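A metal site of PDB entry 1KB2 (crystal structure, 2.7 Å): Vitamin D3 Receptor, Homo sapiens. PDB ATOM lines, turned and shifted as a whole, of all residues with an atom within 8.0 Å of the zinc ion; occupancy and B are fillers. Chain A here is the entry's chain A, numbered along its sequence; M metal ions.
Of the 16 residues printed, 4 come within 4 Å of the zinc ion. The nearest printed residue that does not touch the zinc ion is Pro 46 (4.4 Å).
The side-chain sulfur (SG) of Cys 45 lies close to the backbone NH (N) of Phe 47 (3.5 Å). SG of Cys 45 lies close to N of Gly 49.
The zinc ion is bound by SG of Cys 51 (2.2 Å), SG of Cys 61 (2.2 Å), SG of Cys 45 (2.2 Å) and SG of Cys 64 (2.3 Å).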
ATOM      1  N   THR A  44      21.597 -23.280  28.314  1.00  0.00           N
ATOM      2  CA  THR A  44      22.004 -22.412  27.208  1.00  0.00           C
ATOM      3  C   THR A  44      20.971 -21.334  26.912  1.00  0.00           C
ATOM      4  O   THR A  44      19.832 -21.664  26.572  1.00  0.00           O
ATOM      5  CB  THR A  44      22.247 -23.260  25.902  1.00  0.00           C
ATOM      6  OG1 THR A  44      23.493 -23.964  26.014  1.00  0.00           O
ATOM      7  CG2 THR A  44      22.269 -22.369  24.656  1.00  0.00           C
ATOM      8  N   CYS A  45      21.356 -20.053  27.033  1.00  0.00           N
ATOM      9  CA  CYS A  45      20.448 -18.954  26.766  1.00  0.00           C
ATOM     10  C   CYS A  45      19.944 -18.936  25.304  1.00  0.00           C
ATOM     11  O   CYS A  45      20.719 -19.028  24.374  1.00  0.00           O
ATOM     12  CB  CYS A  45      21.132 -17.650  27.109  1.00  0.00           C
ATOM     13  SG  CYS A  45      20.037 -16.231  27.024  1.00  0.00           S
ATOM     14  N   PRO A  46      18.632 -18.811  25.084  1.00  0.00           N
ATOM     15  CA  PRO A  46      18.082 -18.797  23.710  1.00  0.00           C
ATOM     16  C   PRO A  46      18.193 -17.435  23.047  1.00  0.00           C
ATOM     17  O   PRO A  46      17.880 -17.274  21.858  1.00  0.00           O
ATOM     18  CB  PRO A  46      16.610 -19.161  23.903  1.00  0.00           C
ATOM     19  CG  PRO A  46      16.508 -19.593  25.340  1.00  0.00           C
ATOM     20  CD  PRO A  46      17.557 -18.827  26.070  1.00  0.00           C
ATOM     21  N   PHE A  47      18.611 -16.450  23.819  1.00  0.00           N
ATOM     22  CA  PHE A  47      18.699 -15.098  23.314  1.00  0.00           C
ATOM     23  C   PHE A  47      20.090 -14.538  23.219  1.00  0.00           C
ATOM     24  O   PHE A  47      20.868 -14.968  22.372  1.00  0.00           O
ATOM     25  CB  PHE A  47      17.859 -14.198  24.207  1.00  0.00           C
ATOM     26  CG  PHE A  47      16.469 -14.677  24.370  1.00  0.00           C
ATOM     27  CD1 PHE A  47      15.450 -14.163  23.603  1.00  0.00           C
ATOM     28  CD2 PHE A  47      16.180 -15.687  25.293  1.00  0.00           C
ATOM     29  CE1 PHE A  47      14.145 -14.638  23.751  1.00  0.00           C
ATOM     30  CE2 PHE A  47      14.885 -16.167  25.460  1.00  0.00           C
ATOM     31  CZ  PHE A  47      13.863 -15.644  24.692  1.00  0.00           C
ATOM     32  N   ASN A  48      20.406 -13.604  24.104  1.00  0.00           N
ATOM     33  CA  ASN A  48      21.690 -12.930  24.106  1.00  0.00           C
ATOM     34  C   ASN A  48      22.605 -13.144  25.304  1.00  0.00           C
ATOM     35  O   ASN A  48      23.704 -12.568  25.321  1.00  0.00           O
ATOM     36  CB  ASN A  48      21.478 -11.425  23.929  1.00  0.00           C
ATOM     37  CG  ASN A  48      20.589 -11.115  22.764  1.00  0.00           C
ATOM     38  OD1 ASN A  48      20.942 -11.405  21.620  1.00  0.00           O
ATOM     39  ND2 ASN A  48      19.422 -10.542  23.041  1.00  0.00           N
ATOM     40  N   GLY A  49      22.165 -13.931  26.292  1.00  0.00           N
ATOM     41  CA  GLY A  49      23.033 -14.186  27.442  1.00  0.00           C
ATOM     42  C   GLY A  49      22.973 -13.137  28.529  1.00  0.00           C
ATOM     43  O   GLY A  49      23.734 -13.182  29.506  1.00  0.00           O
ATOM     44  N   ASP A  50      22.083 -12.177  28.390  1.00  0.00           N
ATOM     45  CA  ASP A  50      21.953 -11.156  29.414  1.00  0.00           C
ATOM     46  C   ASP A  50      20.491 -10.854  29.696  1.00  0.00           C
ATOM     47  O   ASP A  50      20.086  -9.672  29.816  1.00  0.00           O
ATOM     48  CB  ASP A  50      22.649  -9.892  28.978  1.00  0.00           C
ATOM     49  CG  ASP A  50      22.306  -9.521  27.583  1.00  0.00           C
ATOM     50  OD1 ASP A  50      21.454 -10.221  26.986  1.00  0.00           O
ATOM     51  OD2 ASP A  50      22.882  -8.543  27.081  1.00  0.00           O
ATOM     52  N   CYS A  51      19.703 -11.933  29.790  1.00  0.00           N
ATOM     53  CA  CYS A  51      18.271 -11.862  30.082  1.00  0.00           C
ATOM     54  C   CYS A  51      18.003 -11.146  31.409  1.00  0.00           C
ATOM     55  O   CYS A  51      18.741 -11.323  32.406  1.00  0.00           O
ATOM     56  CB  CYS A  51      17.678 -13.262  30.148  1.00  0.00           C
ATOM     57  SG  CYS A  51      17.586 -14.198  28.607  1.00  0.00           S
ATOM     58  N   ARG A  52      16.973 -10.310  31.406  1.00  0.00           N
ATOM     59  CA  ARG A  52      16.572  -9.555  32.602  1.00  0.00           C
ATOM     60  C   ARG A  52      15.590 -10.401  33.438  1.00  0.00           C
ATOM     61  O   ARG A  52      14.385 -10.419  33.151  1.00  0.00           O
ATOM     62  CB  ARG A  52      15.934  -8.205  32.223  1.00  0.00           C
ATOM     63  CG  ARG A  52      16.936  -7.170  31.801  1.00  0.00           C
ATOM     64  CD  ARG A  52      16.372  -5.819  31.803  1.00  0.00           C
ATOM     65  NE  ARG A  52      17.326  -4.878  31.235  1.00  0.00           N
ATOM     66  CZ  ARG A  52      17.239  -3.560  31.395  1.00  0.00           C
ATOM     67  NH1 ARG A  52      16.233  -3.037  32.107  1.00  0.00           N
ATOM     68  NH2 ARG A  52      18.175  -2.756  30.880  1.00  0.00           N
ATOM     69  N   ILE A  53      16.108 -11.076  34.452  1.00  0.00           N
ATOM     70  CA  ILE A  53      15.272 -11.966  35.236  1.00  0.00           C
ATOM     71  C   ILE A  53      14.229 -11.289  36.116  1.00  0.00           C
ATOM     72  O   ILE A  53      14.516 -10.349  36.855  1.00  0.00           O
ATOM     73  CB  ILE A  53      16.154 -12.901  36.111  1.00  0.00           C
ATOM     74  CG1 ILE A  53      17.192 -13.640  35.260  1.00  0.00           C
ATOM     75  CG2 ILE A  53      15.267 -13.924  36.794  1.00  0.00           C
ATOM     76  CD1 ILE A  53      16.548 -14.487  34.173  1.00  0.00           C
ATOM     77  N   HIS A  60      11.742 -18.993  32.028  1.00  0.00           N
ATOM     78  CA  HIS A  60      12.063 -18.903  30.603  1.00  0.00           C
ATOM     79  C   HIS A  60      13.567 -18.982  30.314  1.00  0.00           C
ATOM     80  O   HIS A  60      13.976 -19.576  29.310  1.00  0.00           O
ATOM     81  CB  HIS A  60      11.479 -17.627  29.973  1.00  0.00           C
ATOM     82  CG  HIS A  60       9.972 -17.505  30.096  1.00  0.00           C
ATOM     83  ND1 HIS A  60       9.121 -18.601  30.009  1.00  0.00           N
ATOM     84  CD2 HIS A  60       9.186 -16.427  30.340  1.00  0.00           C
ATOM     85  CE1 HIS A  60       7.870 -18.191  30.195  1.00  0.00           C
ATOM     86  NE2 HIS A  60       7.888 -16.878  30.401  1.00  0.00           N
ATOM     87  N   CYS A  61      14.418 -18.375  31.114  1.00  0.00           N
ATOM     88  CA  CYS A  61      15.802 -18.579  30.797  1.00  0.00           C
ATOM     89  C   CYS A  61      16.591 -19.151  31.970  1.00  0.00           C
ATOM     90  O   CYS A  61      17.079 -18.407  32.849  1.00  0.00           O
ATOM     91  CB  CYS A  61      16.470 -17.311  30.284  1.00  0.00           C
ATOM     92  SG  CYS A  61      18.194 -17.687  29.637  1.00  0.00           S
ATOM     93  N   GLN A  62      16.733 -20.474  31.987  1.00  0.00           N
ATOM     94  CA  GLN A  62      17.488 -21.100  33.065  1.00  0.00           C
ATOM     95  C   GLN A  62      18.962 -20.730  33.015  1.00  0.00           C
ATOM     96  O   GLN A  62      19.569 -20.477  34.064  1.00  0.00           O
ATOM     97  CB  GLN A  62      17.323 -22.591  33.000  1.00  0.00           C
ATOM     98  CG  GLN A  62      16.043 -22.891  32.368  1.00  0.00           C
ATOM     99  CD  GLN A  62      15.721 -24.336  32.405  1.00  0.00           C
ATOM    100  OE1 GLN A  62      16.369 -25.166  31.735  1.00  0.00           O
ATOM    101  NE2 GLN A  62      14.697 -24.685  33.183  1.00  0.00           N
ATOM    102  N   ALA A  63      19.546 -20.679  31.820  1.00  0.00           N
ATOM    103  CA  ALA A  63      20.954 -20.324  31.724  1.00  0.00           C
ATOM    104  C   ALA A  63      21.213 -19.037  32.446  1.00  0.00           C
ATOM    105  O   ALA A  63      22.107 -18.960  33.290  1.00  0.00           O
ATOM    106  CB  ALA A  63      21.360 -20.174  30.314  1.00  0.00           C
ATOM    107  N   CYS A  64      20.391 -18.020  32.151  1.00  0.00           N
ATOM    108  CA  CYS A  64      20.570 -16.713  32.791  1.00  0.00           C
ATOM    109  C   CYS A  64      20.211 -16.728  34.248  1.00  0.00           C
ATOM    110  O   CYS A  64      20.936 -16.110  35.033  1.00  0.00           O
ATOM    111  CB  CYS A  64      19.783 -15.596  32.065  1.00  0.00           C
ATOM    112  SG  CYS A  64      20.534 -15.031  30.481  1.00  0.00           S
ATOM    113  N   ARG A  65      19.143 -17.420  34.625  1.00  0.00           N
ATOM    114  CA  ARG A  65      18.788 -17.491  36.038  1.00  0.00           C
ATOM    115  C   ARG A  65      19.948 -18.100  36.880  1.00  0.00           C
ATOM    116  O   ARG A  65      20.341 -17.554  37.949  1.00  0.00           O
ATOM    117  CB  ARG A  65      17.572 -18.357  36.211  1.00  0.00           C
ATOM    118  CG  ARG A  65      16.948 -18.274  37.579  1.00  0.00           C
ATOM    119  CD  ARG A  65      15.753 -19.127  37.616  1.00  0.00           C
ATOM    120  NE  ARG A  65      15.002 -19.066  38.856  1.00  0.00           N
ATOM    121  CZ  ARG A  65      13.903 -19.798  39.056  1.00  0.00           C
ATOM    122  NH1 ARG A  65      13.487 -20.604  38.082  1.00  0.00           N
ATOM    123  NH2 ARG A  65      13.232 -19.747  40.174  1.00  0.00           N
HETATM  124 ZN    ZN M   1      19.009 -15.790  28.961  1.00  0.00          ZN
